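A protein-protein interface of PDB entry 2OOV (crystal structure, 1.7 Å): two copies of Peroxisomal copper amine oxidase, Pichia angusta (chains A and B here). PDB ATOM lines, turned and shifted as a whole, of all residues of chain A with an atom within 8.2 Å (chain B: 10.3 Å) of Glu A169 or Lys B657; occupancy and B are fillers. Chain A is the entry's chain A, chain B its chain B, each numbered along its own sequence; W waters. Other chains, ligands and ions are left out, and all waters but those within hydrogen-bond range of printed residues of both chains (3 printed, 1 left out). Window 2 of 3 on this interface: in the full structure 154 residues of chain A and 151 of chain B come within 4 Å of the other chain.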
ATOM      1  N   HIS A 137       7.869 -17.989  16.834  1.00  0.00           N
ATOM      2  CA  HIS A 137       6.791 -18.998  16.753  1.00  0.00           C
ATOM      3  C   HIS A 137       5.473 -18.422  16.203  1.00  0.00           C
ATOM      4  O   HIS A 137       4.568 -19.181  15.813  1.00  0.00           O
ATOM      5  CB  HIS A 137       6.555 -19.683  18.113  1.00  0.00           C
ATOM      6  CG  HIS A 137       5.773 -18.855  19.089  1.00  0.00           C
ATOM      7  ND1 HIS A 137       6.369 -17.973  19.970  1.00  0.00           N
ATOM      8  CD2 HIS A 137       4.441 -18.780  19.329  1.00  0.00           C
ATOM      9  CE1 HIS A 137       5.438 -17.379  20.697  1.00  0.00           C
ATOM     10  NE2 HIS A 137       4.260 -17.854  20.331  1.00  0.00           N
ATOM     11  N   LYS A 138       5.373 -17.093  16.183  1.00  0.00           N
ATOM     12  CA  LYS A 138       4.191 -16.378  15.697  1.00  0.00           C
ATOM     13  C   LYS A 138       4.302 -16.045  14.202  1.00  0.00           C
ATOM     14  O   LYS A 138       3.360 -15.497  13.605  1.00  0.00           O
ATOM     15  CB  LYS A 138       4.008 -15.072  16.479  1.00  0.00           C
ATOM     16  CG  LYS A 138       3.625 -15.258  17.950  1.00  0.00           C
ATOM     17  CD  LYS A 138       3.222 -13.946  18.599  1.00  0.00           C
ATOM     18  CE  LYS A 138       2.857 -14.150  20.077  1.00  0.00           C
ATOM     19  NZ  LYS A 138       2.822 -12.838  20.821  1.00  0.00           N
ATOM     20  N   TYR A 140       4.728 -17.190  10.350  1.00  0.00           N
ATOM     21  CA  TYR A 140       4.343 -18.310   9.506  1.00  0.00           C
ATOM     22  C   TYR A 140       4.679 -17.985   8.055  1.00  0.00           C
ATOM     23  O   TYR A 140       4.915 -16.822   7.706  1.00  0.00           O
ATOM     24  CB  TYR A 140       2.836 -18.574   9.638  1.00  0.00           C
ATOM     25  CG  TYR A 140       2.404 -19.139  10.986  1.00  0.00           C
ATOM     26  CD1 TYR A 140       2.339 -18.326  12.113  1.00  0.00           C
ATOM     27  CD2 TYR A 140       2.042 -20.486  11.114  1.00  0.00           C
ATOM     28  CE1 TYR A 140       1.941 -18.834  13.353  1.00  0.00           C
ATOM     29  CE2 TYR A 140       1.642 -21.003  12.349  1.00  0.00           C
ATOM     30  CZ  TYR A 140       1.595 -20.174  13.455  1.00  0.00           C
ATOM     31  OH  TYR A 140       1.191 -20.678  14.675  1.00  0.00           O
ATOM     32  N   ARG A 166       0.753 -14.435  13.023  1.00  0.00           N
ATOM     33  CA  ARG A 166      -0.432 -14.745  13.826  1.00  0.00           C
ATOM     34  C   ARG A 166      -0.222 -14.298  15.272  1.00  0.00           C
ATOM     35  O   ARG A 166       0.807 -14.640  15.870  1.00  0.00           O
ATOM     36  CB  ARG A 166      -0.697 -16.249  13.829  1.00  0.00           C
ATOM     37  CG  ARG A 166      -1.030 -16.845  12.471  1.00  0.00           C
ATOM     38  CD  ARG A 166      -1.478 -18.291  12.610  1.00  0.00           C
ATOM     39  NE  ARG A 166      -1.291 -19.034  11.360  1.00  0.00           N
ATOM     40  CZ  ARG A 166      -1.553 -20.335  11.219  1.00  0.00           C
ATOM     41  NH1 ARG A 166      -2.005 -21.038  12.260  1.00  0.00           N
ATOM     42  NH2 ARG A 166      -1.355 -20.940  10.057  1.00  0.00           N
ATOM     43  N   SER A 167      -1.180 -13.543  15.816  1.00  0.00           N
ATOM     44  CA  SER A 167      -1.135 -13.129  17.223  1.00  0.00           C
ATOM     45  C   SER A 167      -1.464 -14.313  18.130  1.00  0.00           C
ATOM     46  O   SER A 167      -0.969 -14.399  19.265  1.00  0.00           O
ATOM     47  CB  SER A 167      -2.102 -11.971  17.489  1.00  0.00           C
ATOM     48  OG  SER A 167      -3.451 -12.398  17.413  1.00  0.00           O
ATOM     49  N   ASP A 168      -2.285 -15.225  17.608  1.00  0.00           N
ATOM     50  CA  ASP A 168      -2.714 -16.432  18.293  1.00  0.00           C
ATOM     51  C   ASP A 168      -2.747 -17.528  17.235  1.00  0.00           C
ATOM     52  O   ASP A 168      -3.063 -17.252  16.071  1.00  0.00           O
ATOM     53  CB  ASP A 168      -4.110 -16.229  18.900  1.00  0.00           C
ATOM     54  CG  ASP A 168      -4.634 -17.476  19.585  1.00  0.00           C
ATOM     55  OD1 ASP A 168      -4.283 -17.703  20.762  1.00  0.00           O
ATOM     56  OD2 ASP A 168      -5.386 -18.237  18.942  1.00  0.00           O
ATOM     57  N   GLU A 169      -2.420 -18.758  17.622  1.00  0.00           N
ATOM     58  CA  GLU A 169      -2.339 -19.864  16.676  1.00  0.00           C
ATOM     59  C   GLU A 169      -3.632 -20.136  15.885  1.00  0.00           C
ATOM     60  O   GLU A 169      -3.577 -20.736  14.810  1.00  0.00           O
ATOM     61  CB  GLU A 169      -1.859 -21.152  17.358  1.00  0.00           C
ATOM     62  CG  GLU A 169      -2.860 -21.736  18.332  1.00  0.00           C
ATOM     63  CD  GLU A 169      -2.326 -22.918  19.134  1.00  0.00           C
ATOM     64  OE1 GLU A 169      -1.347 -23.563  18.699  1.00  0.00           O
ATOM     65  OE2 GLU A 169      -2.920 -23.201  20.200  1.00  0.00           O
ATOM     66  N   ASP A 170      -4.775 -19.710  16.425  1.00  0.00           N
ATOM     67  CA  ASP A 170      -6.073 -19.958  15.784  1.00  0.00           C
ATOM     68  C   ASP A 170      -6.478 -18.841  14.814  1.00  0.00           C
ATOM     69  O   ASP A 170      -7.507 -18.947  14.137  1.00  0.00           O
ATOM     70  CB  ASP A 170      -7.175 -20.142  16.835  1.00  0.00           C
ATOM     71  CG  ASP A 170      -7.035 -21.434  17.632  1.00  0.00           C
ATOM     72  OD1 ASP A 170      -6.266 -22.326  17.238  1.00  0.00           O
ATOM     73  OD2 ASP A 170      -7.736 -21.546  18.666  1.00  0.00           O
ATOM     74  N   ASP A 171      -5.690 -17.764  14.770  1.00  0.00           N
ATOM     75  CA  ASP A 171      -5.901 -16.665  13.812  1.00  0.00           C
ATOM     76  C   ASP A 171      -5.836 -17.158  12.383  1.00  0.00           C
ATOM     77  O   ASP A 171      -5.129 -18.113  12.081  1.00  0.00           O
ATOM     78  CB  ASP A 171      -4.818 -15.602  13.962  1.00  0.00           C
ATOM     79  CG  ASP A 171      -4.997 -14.744  15.187  1.00  0.00           C
ATOM     80  OD1 ASP A 171      -6.090 -14.738  15.797  1.00  0.00           O
ATOM     81  OD2 ASP A 171      -4.024 -14.059  15.538  1.00  0.00           O
ATOM     82  N   SER A 172      -6.572 -16.487  11.500  1.00  0.00           N
ATOM     83  CA  SER A 172      -6.260 -16.550  10.081  1.00  0.00           C
ATOM     84  C   SER A 172      -5.160 -15.518   9.780  1.00  0.00           C
ATOM     85  O   SER A 172      -5.349 -14.307   9.982  1.00  0.00           O
ATOM     86  CB  SER A 172      -7.500 -16.289   9.234  1.00  0.00           C
ATOM     87  OG  SER A 172      -7.198 -16.574   7.881  1.00  0.00           O
ATOM     88  N   GLN A 173      -4.016 -16.001   9.294  1.00  0.00           N
ATOM     89  CA  GLN A 173      -2.811 -15.179   9.220  1.00  0.00           C
ATOM     90  C   GLN A 173      -2.857 -14.099   8.143  1.00  0.00           C
ATOM     91  O   GLN A 173      -2.055 -13.155   8.148  1.00  0.00           O
ATOM     92  CB  GLN A 173      -1.577 -16.060   9.005  1.00  0.00           C
ATOM     93  CG  GLN A 173      -1.514 -16.732   7.637  1.00  0.00           C
ATOM     94  CD  GLN A 173      -0.562 -17.924   7.616  1.00  0.00           C
ATOM     95  OE1 GLN A 173      -0.307 -18.536   8.643  1.00  0.00           O
ATOM     96  NE2 GLN A 173      -0.062 -18.268   6.439  1.00  0.00           N
ATOM     97  N   ASN A 210     -10.721 -12.625  11.499  1.00  0.00           N
ATOM     98  CA  ASN A 210     -10.955 -14.024  11.786  1.00  0.00           C
ATOM     99  C   ASN A 210     -12.366 -14.485  11.396  1.00  0.00           C
ATOM    100  O   ASN A 210     -13.237 -13.653  11.144  1.00  0.00           O
ATOM    101  CB  ASN A 210     -10.614 -14.298  13.256  1.00  0.00           C
ATOM    102  CG  ASN A 210      -9.106 -14.317  13.506  1.00  0.00           C
ATOM    103  OD1 ASN A 210      -8.323 -14.694  12.630  1.00  0.00           O
ATOM    104  ND2 ASN A 210      -8.696 -13.912  14.707  1.00  0.00           N
ATOM    105  N   TYR A 212     -13.788 -18.120  12.528  1.00  0.00           N
ATOM    106  CA  TYR A 212     -14.404 -19.213  13.298  1.00  0.00           C
ATOM    107  C   TYR A 212     -15.530 -18.658  14.190  1.00  0.00           C
ATOM    108  O   TYR A 212     -15.532 -17.467  14.520  1.00  0.00           O
ATOM    109  CB  TYR A 212     -13.356 -19.970  14.137  1.00  0.00           C
ATOM    110  CG  TYR A 212     -12.570 -21.003  13.349  1.00  0.00           C
ATOM    111  CD1 TYR A 212     -11.483 -20.630  12.544  1.00  0.00           C
ATOM    112  CD2 TYR A 212     -12.916 -22.358  13.402  1.00  0.00           C
ATOM    113  CE1 TYR A 212     -10.774 -21.588  11.823  1.00  0.00           C
ATOM    114  CE2 TYR A 212     -12.213 -23.314  12.689  1.00  0.00           C
ATOM    115  CZ  TYR A 212     -11.138 -22.925  11.903  1.00  0.00           C
ATOM    116  OH  TYR A 212     -10.441 -23.867  11.195  1.00  0.00           O
ATOM    117  N   LYS A 214     -16.179 -18.663  17.332  1.00  0.00           N
ATOM    118  CA  LYS A 214     -15.767 -17.930  18.529  1.00  0.00           C
ATOM    119  C   LYS A 214     -15.358 -16.494  18.175  1.00  0.00           C
ATOM    120  O   LYS A 214     -15.710 -15.558  18.887  1.00  0.00           O
ATOM    121  CB  LYS A 214     -14.684 -18.686  19.317  1.00  0.00           C
ATOM    122  CG  LYS A 214     -13.349 -18.882  18.597  1.00  0.00           C
ATOM    123  CD  LYS A 214     -12.286 -19.363  19.578  1.00  0.00           C
ATOM    124  CE  LYS A 214     -10.909 -19.395  18.928  1.00  0.00           C
ATOM    125  NZ  LYS A 214      -9.915 -20.167  19.740  1.00  0.00           N
ATOM    126  N   HIS A 215     -14.656 -16.329  17.049  1.00  0.00           N
ATOM    127  CA  HIS A 215     -14.277 -14.996  16.564  1.00  0.00           C
ATOM    128  C   HIS A 215     -15.474 -14.151  16.132  1.00  0.00           C
ATOM    129  O   HIS A 215     -15.504 -12.937  16.359  1.00  0.00           O
ATOM    130  CB  HIS A 215     -13.308 -15.089  15.379  1.00  0.00           C
ATOM    131  CG  HIS A 215     -12.111 -15.953  15.617  1.00  0.00           C
ATOM    132  ND1 HIS A 215     -11.845 -17.067  14.853  1.00  0.00           N
ATOM    133  CD2 HIS A 215     -11.079 -15.841  16.492  1.00  0.00           C
ATOM    134  CE1 HIS A 215     -10.711 -17.615  15.253  1.00  0.00           C
ATOM    135  NE2 HIS A 215     -10.229 -16.892  16.250  1.00  0.00           N
ATOM    136  N   ASP B 366      -6.077 -25.729   6.906  1.00  0.00           N
ATOM    137  CA  ASP B 366      -4.645 -25.414   7.031  1.00  0.00           C
ATOM    138  C   ASP B 366      -3.800 -26.667   6.747  1.00  0.00           C
ATOM    139  O   ASP B 366      -3.918 -27.658   7.471  1.00  0.00           O
ATOM    140  CB  ASP B 366      -4.379 -24.882   8.445  1.00  0.00           C
ATOM    141  CG  ASP B 366      -3.013 -24.217   8.602  1.00  0.00           C
ATOM    142  OD1 ASP B 366      -2.085 -24.524   7.825  1.00  0.00           O
ATOM    143  OD2 ASP B 366      -2.886 -23.395   9.542  1.00  0.00           O
ATOM    144  N   ARG B 368      -0.801 -27.180   7.413  1.00  0.00           N
ATOM    145  CA  ARG B 368       0.217 -27.384   8.457  1.00  0.00           C
ATOM    146  C   ARG B 368      -0.023 -28.586   9.363  1.00  0.00           C
ATOM    147  O   ARG B 368       0.934 -29.255   9.758  1.00  0.00           O
ATOM    148  CB  ARG B 368       0.404 -26.115   9.282  1.00  0.00           C
ATOM    149  CG  ARG B 368       1.093 -25.022   8.485  1.00  0.00           C
ATOM    150  CD  ARG B 368       0.998 -23.667   9.151  1.00  0.00           C
ATOM    151  NE  ARG B 368       1.541 -22.643   8.260  1.00  0.00           N
ATOM    152  CZ  ARG B 368       0.858 -22.060   7.281  1.00  0.00           C
ATOM    153  NH1 ARG B 368      -0.416 -22.381   7.067  1.00  0.00           N
ATOM    154  NH2 ARG B 368       1.448 -21.144   6.518  1.00  0.00           N
ATOM    155  N   ASP B 369      -1.289 -28.847   9.694  1.00  0.00           N
ATOM    156  CA  ASP B 369      -1.668 -30.018  10.490  1.00  0.00           C
ATOM    157  C   ASP B 369      -2.507 -31.000   9.676  1.00  0.00           C
ATOM    158  O   ASP B 369      -3.444 -31.622  10.192  1.00  0.00           O
ATOM    159  CB  ASP B 369      -2.370 -29.619  11.790  1.00  0.00           C
ATOM    160  CG  ASP B 369      -3.667 -28.852  11.569  1.00  0.00           C
ATOM    161  OD1 ASP B 369      -4.174 -28.777  10.423  1.00  0.00           O
ATOM    162  OD2 ASP B 369      -4.182 -28.319  12.567  1.00  0.00           O
ATOM    163  N   ASN B 370      -2.154 -31.124   8.400  1.00  0.00           N
ATOM    164  CA  ASN B 370      -2.840 -32.009   7.472  1.00  0.00           C
ATOM    165  C   ASN B 370      -4.354 -31.764   7.367  1.00  0.00           C
ATOM    166  O   ASN B 370      -5.158 -32.713   7.315  1.00  0.00           O
ATOM    167  CB  ASN B 370      -2.555 -33.471   7.821  1.00  0.00           C
ATOM    168  CG  ASN B 370      -2.849 -34.389   6.672  1.00  0.00           C
ATOM    169  OD1 ASN B 370      -2.456 -34.112   5.537  1.00  0.00           O
ATOM    170  ND2 ASN B 370      -3.564 -35.482   6.943  1.00  0.00           N
ATOM    171  N   PHE B 371      -4.734 -30.487   7.352  1.00  0.00           N
ATOM    172  CA  PHE B 371      -6.139 -30.072   7.226  1.00  0.00           C
ATOM    173  C   PHE B 371      -7.032 -30.384   8.438  1.00  0.00           C
ATOM    174  O   PHE B 371      -8.262 -30.278   8.355  1.00  0.00           O
ATOM    175  CB  PHE B 371      -6.756 -30.615   5.931  1.00  0.00           C
ATOM    176  CG  PHE B 371      -5.882 -30.444   4.729  1.00  0.00           C
ATOM    177  CD1 PHE B 371      -5.434 -29.180   4.336  1.00  0.00           C
ATOM    178  CD2 PHE B 371      -5.506 -31.547   3.975  1.00  0.00           C
ATOM    179  CE1 PHE B 371      -4.622 -29.026   3.217  1.00  0.00           C
ATOM    180  CE2 PHE B 371      -4.697 -31.404   2.848  1.00  0.00           C
ATOM    181  CZ  PHE B 371      -4.249 -30.145   2.467  1.00  0.00           C
ATOM    182  N   ALA B 372      -6.423 -30.748   9.570  1.00  0.00           N
ATOM    183  CA  ALA B 372      -7.178 -30.926  10.805  1.00  0.00           C
ATOM    184  C   ALA B 372      -7.838 -29.604  11.192  1.00  0.00           C
ATOM    185  O   ALA B 372      -8.981 -29.584  11.643  1.00  0.00           O
ATOM    186  CB  ALA B 372      -6.274 -31.440  11.927  1.00  0.00           C
ATOM    187  N   THR B 373      -7.099 -28.505  11.019  1.00  0.00           N
ATOM    188  CA  THR B 373      -7.648 -27.159  11.126  1.00  0.00           C
ATOM    189  C   THR B 373      -8.475 -26.960   9.858  1.00  0.00           C
ATOM    190  O   THR B 373      -7.943 -26.990   8.751  1.00  0.00           O
ATOM    191  CB  THR B 373      -6.529 -26.098  11.208  1.00  0.00           C
ATOM    192  OG1 THR B 373      -5.855 -26.218  12.468  1.00  0.00           O
ATOM    193  CG2 THR B 373      -7.101 -24.678  11.110  1.00  0.00           C
ATOM    194  N   SER B 374      -9.781 -26.827  10.038  1.00  0.00           N
ATOM    195  CA  SER B 374     -10.713 -26.818   8.906  1.00  0.00           C
ATOM    196  C   SER B 374     -12.043 -26.206   9.298  1.00  0.00           C
ATOM    197  O   SER B 374     -12.542 -26.425  10.407  1.00  0.00           O
ATOM    198  CB  SER B 374     -10.943 -28.240   8.391  1.00  0.00           C
ATOM    199  OG  SER B 374     -11.573 -28.224   7.114  1.00  0.00           O
ATOM    200  N   TYR B 649     -18.927 -27.997   9.862  1.00  0.00           N
ATOM    201  CA  TYR B 649     -17.808 -28.533  10.621  1.00  0.00           C
ATOM    202  C   TYR B 649     -16.806 -27.421  10.850  1.00  0.00           C
ATOM    203  O   TYR B 649     -16.502 -26.654   9.930  1.00  0.00           O
ATOM    204  CB  TYR B 649     -17.140 -29.704   9.886  1.00  0.00           C
ATOM    205  CG  TYR B 649     -15.980 -30.296  10.658  1.00  0.00           C
ATOM    206  CD1 TYR B 649     -16.211 -31.149  11.733  1.00  0.00           C
ATOM    207  CD2 TYR B 649     -14.657 -29.985  10.329  1.00  0.00           C
ATOM    208  CE1 TYR B 649     -15.159 -31.692  12.461  1.00  0.00           C
ATOM    209  CE2 TYR B 649     -13.591 -30.522  11.055  1.00  0.00           C
ATOM    210  CZ  TYR B 649     -13.857 -31.376  12.123  1.00  0.00           C
ATOM    211  OH  TYR B 649     -12.835 -31.917  12.862  1.00  0.00           O
ATOM    212  N   MET B 651     -13.055 -26.967  13.159  1.00  0.00           N
ATOM    213  CA  MET B 651     -12.017 -27.299  14.122  1.00  0.00           C
ATOM    214  C   MET B 651     -10.850 -26.323  13.997  1.00  0.00           C
ATOM    215  O   MET B 651     -10.299 -26.137  12.905  1.00  0.00           O
ATOM    216  CB  MET B 651     -11.522 -28.728  13.927  1.00  0.00           C
ATOM    217  CG  MET B 651     -10.306 -29.043  14.806  1.00  0.00           C
ATOM    218  SD  MET B 651      -9.986 -30.781  15.045  1.00  0.00           S
ATOM    219  CE  MET B 651     -11.483 -31.307  15.898  1.00  0.00           C
ATOM    220  N   THR B 652     -10.479 -25.716  15.123  1.00  0.00           N
ATOM    221  CA  THR B 652      -9.349 -24.791  15.173  1.00  0.00           C
ATOM    222  C   THR B 652      -8.020 -25.516  15.368  1.00  0.00           C
ATOM    223  O   THR B 652      -7.986 -26.716  15.675  1.00  0.00           O
ATOM    224  CB  THR B 652      -9.502 -23.737  16.281  1.00  0.00           C
ATOM    225  OG1 THR B 652      -9.407 -24.375  17.566  1.00  0.00           O
ATOM    226  CG2 THR B 652     -10.821 -23.009  16.168  1.00  0.00           C
ATOM    227  N   THR B 653      -6.925 -24.786  15.168  1.00  0.00           N
ATOM    228  CA  THR B 653      -5.591 -25.329  15.386  1.00  0.00           C
ATOM    229  C   THR B 653      -5.414 -25.833  16.821  1.00  0.00           C
ATOM    230  O   THR B 653      -4.934 -26.954  17.018  1.00  0.00           O
ATOM    231  CB  THR B 653      -4.509 -24.308  15.005  1.00  0.00           C
ATOM    232  OG1 THR B 653      -4.652 -23.992  13.617  1.00  0.00           O
ATOM    233  CG2 THR B 653      -3.103 -24.868  15.240  1.00  0.00           C
ATOM    234  N   SER B 654      -5.827 -25.018  17.794  1.00  0.00           N
ATOM    235  CA  SER B 654      -5.709 -25.367  19.211  1.00  0.00           C
ATOM    236  C   SER B 654      -6.563 -26.576  19.569  1.00  0.00           C
ATOM    237  O   SER B 654      -6.113 -27.462  20.298  1.00  0.00           O
ATOM    238  CB  SER B 654      -6.034 -24.183  20.118  1.00  0.00           C
ATOM    239  OG  SER B 654      -7.386 -23.759  20.012  1.00  0.00           O
ATOM    240  N   GLU B 655      -7.786 -26.620  19.032  1.00  0.00           N
ATOM    241  CA  GLU B 655      -8.656 -27.776  19.215  1.00  0.00           C
ATOM    242  C   GLU B 655      -8.042 -29.023  18.594  1.00  0.00           C
ATOM    243  O   GLU B 655      -8.110 -30.105  19.186  1.00  0.00           O
ATOM    244  CB  GLU B 655     -10.039 -27.527  18.621  1.00  0.00           C
ATOM    245  CG  GLU B 655     -10.913 -26.641  19.461  1.00  0.00           C
ATOM    246  CD  GLU B 655     -12.137 -26.161  18.710  1.00  0.00           C
ATOM    247  OE1 GLU B 655     -12.284 -26.490  17.502  1.00  0.00           O
ATOM    248  OE2 GLU B 655     -12.947 -25.438  19.330  1.00  0.00           O
ATOM    249  N   ALA B 656      -7.441 -28.873  17.413  1.00  0.00           N
ATOM    250  CA  ALA B 656      -6.792 -29.995  16.734  1.00  0.00           C
ATOM    251  C   ALA B 656      -5.595 -30.530  17.529  1.00  0.00           C
ATOM    252  O   ALA B 656      -5.323 -31.733  17.515  1.00  0.00           O
ATOM    253  CB  ALA B 656      -6.370 -29.613  15.319  1.00  0.00           C
ATOM    254  N   LYS B 657      -4.888 -29.628  18.208  1.00  0.00           N
ATOM    255  CA  LYS B 657      -3.761 -29.998  19.073  1.00  0.00           C
ATOM    256  C   LYS B 657      -4.240 -30.750  20.317  1.00  0.00           C
ATOM    257  O   LYS B 657      -3.607 -31.713  20.738  1.00  0.00           O
ATOM    258  CB  LYS B 657      -2.970 -28.760  19.500  1.00  0.00           C
ATOM    259  CG  LYS B 657      -1.876 -28.303  18.549  1.00  0.00           C
ATOM    260  CD  LYS B 657      -1.333 -26.953  19.014  1.00  0.00           C
ATOM    261  CE  LYS B 657       0.119 -26.736  18.610  1.00  0.00           C
ATOM    262  NZ  LYS B 657       0.331 -26.721  17.131  1.00  0.00           N
ATOM    263  N   ARG B 658      -5.349 -30.301  20.905  1.00  0.00           N
ATOM    264  CA  ARG B 658      -5.933 -30.960  22.077  1.00  0.00           C
ATOM    265  C   ARG B 658      -6.388 -32.396  21.796  1.00  0.00           C
ATOM    266  O   ARG B 658      -6.570 -33.183  22.725  1.00  0.00           O
ATOM    267  CB  ARG B 658      -7.109 -30.151  22.625  1.00  0.00           C
ATOM    268  CG  ARG B 658      -6.739 -29.096  23.647  1.00  0.00           C
ATOM    269  CD  ARG B 658      -7.948 -28.231  23.980  1.00  0.00           C
ATOM    270  NE  ARG B 658      -7.989 -27.000  23.185  1.00  0.00           N
ATOM    271  CZ  ARG B 658      -9.105 -26.366  22.825  1.00  0.00           C
ATOM    272  NH1 ARG B 658     -10.294 -26.852  23.166  1.00  0.00           N
ATOM    273  NH2 ARG B 658      -9.036 -25.243  22.108  1.00  0.00           N
ATOM    274  N   ALA B 659      -6.565 -32.734  20.519  1.00  0.00           N
ATOM    275  CA  ALA B 659      -7.057 -34.053  20.124  1.00  0.00           C
ATOM    276  C   ALA B 659      -6.042 -34.875  19.323  1.00  0.00           C
ATOM    277  O   ALA B 659      -6.399 -35.535  18.338  1.00  0.00           O
ATOM    278  CB  ALA B 659      -8.365 -33.914  19.350  1.00  0.00           C
ATOM    279  N   VAL B 660      -4.780 -34.835  19.738  1.00  0.00           N
ATOM    280  CA  VAL B 660      -3.752 -35.684  19.127  1.00  0.00           C
ATOM    281  C   VAL B 660      -2.859 -36.338  20.173  1.00  0.00           C
ATOM    282  O   VAL B 660      -2.538 -35.743  21.209  1.00  0.00           O
ATOM    283  CB  VAL B 660      -2.871 -34.936  18.081  1.00  0.00           C
ATOM    284  CG1 VAL B 660      -3.538 -34.931  16.713  1.00  0.00           C
ATOM    285  CG2 VAL B 660      -2.528 -33.527  18.539  1.00  0.00           C
ATOM    286  OXT VAL B 660      -2.442 -37.483  19.994  1.00  0.00           O
HETATM  287  O   HOH W   1     -10.769 -23.023  19.520  1.00  0.00           O
HETATM  288  O   HOH W   2      -7.643 -22.325  13.747  1.00  0.00           O
HETATM  289  O   HOH W   3      -2.340 -23.975  12.048  1.00  0.00           O
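Water W3 lies within hydrogen-bond range of the side-chain carboxylate (OD2) of Asp B366, the side-chain hydroxyl (OG1) of Thr B653 and the guanidinium group (NH1) of Arg A166. Water W1 lies within hydrogen-bond range of OG1 of Thr B652 (2.7 Å), NZ of Lys A214 (3.0 Å), OE2 of Glu B655 (3.3 Å), OD2 of Asp A170 (3.5 Å) and OG of Ser B654 (3.5 Å). Water W2 bridges the backbone NH of Thr B653 (2.9 Å) and the backbone carbonyl oxygen of Asp A170 (3.4 Å).
No position is printed for both chains. Of the 14 pairs that touch across the chains among the printed residues, none has its exchanged pair printed and touching as well.
Among the printed residues, merely in contact across the chains: Glu A169 with Ser B654 (3.3 Å), Tyr A212 with Thr B373 (3.4 Å), Tyr A212 with Thr B652 (3.5 Å), Tyr A140 with Arg B368 (3.6 Å) and Glu A169 with Thr B653 (3.6 Å).
NH2 of Arg A166 lies within salt-bridge range of OD2 of Asp B366, 2.9 Å away. The side-chain amino group of Lys B657 is in salt-bridge range of the side-chain carboxylate of Glu A169 (3.9 Å). The side-chain carboxylate (OD2) of Asp A170 lies within hydrogen-bond range of the side-chain hydroxyl (OG1) of Thr B652 (3.5 Å). The side-chain carboxylate of Asp A170 sits at hydrogen-bond distance from the backbone NH of Thr B653 (3.3 Å). The side-chain carboxylate of Asp A170 lies within hydrogen-bond range of the side-chain hydroxyl of Ser B654, at 2.6 Å. NH2 of Arg B368 lies close to NE2 of Gln A173 (3.2 Å). The backbone NH of Ser B374 lies within hydrogen-bond range of the side-chain hydroxyl of Tyr A212. The side-chain hydroxyl of Tyr A212 is in hydrogen-bond range of the backbone carbonyl oxygen of Met B651 (2.8 Å). The guanidinium group (NH2) of Arg A166 sits close to the guanidinium group (NH1) of Arg B368 (3.4 Å).
O of Lys A138 lies within hydrogen-bond range of N of Arg A166, at 2.9 Å. NZ of Lys A214 is in salt-bridge range of OD2 of Asp A170. The side-chain carboxylate (OD2) of Asp B369 is in hydrogen-bond range of the side-chain hydroxyl (OG1) of Thr B373 (2.7 Å). O of Ser B374 sits at hydrogen-bond distance from N of Met B651 (2.9 Å). The side-chain hydroxyl (OG) of Ser B654 is in hydrogen-bond range of the side-chain hydroxyl (OG1) of Thr B652, 3.2 Å away. OG of Ser B654 is in hydrogen-bond range of NH2 of Arg B658.
Of the 19 printed residues of chain B, 9 touch a printed residue of chain A. Among the printed residues, Asp or Glu carboxylates within 4 Å of a Lys or Arg side-chain nitrogen of the other chain: Arg A166 with Asp B366 and Glu A169 with Lys B657.
Glu A169 touches three residues of chain B. Lys B657 touches just one residue of chain A: Glu A169 (3.4 Å). Of chain B, only Thr B652, Thr B653 and Ser B654 come within 4 Å of Asp A170. No residue of chain B comes within 4 Å of Asp A171. Of the printed residues of chain A, Asp B366 touches Arg A166. Of the printed residues of chain B, Tyr A212 touches Thr B373, Ser B374, Met B651 and Thr B652. Of the printed residues of chain A, Arg B368 touches Tyr A140 (3.6 Å), Arg A166 (3.4 Å) and Gln A173 (3.2 Å). Of the printed residues of chain A, Thr B652 touches Asp A170 (3.5 Å) and Tyr A212 (3.5 Å). Of the printed residues of chain A, Thr B373 touches Tyr A212 (3.4 Å). Ser A172 touches none of the printed residues of chain B. The nearest residue of chain A that does not touch Lys B657 is Tyr A140 (6.6 Å). The nearest printed residue of chain A that does not touch Thr B652 is Lys A214 (4.5 Å).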
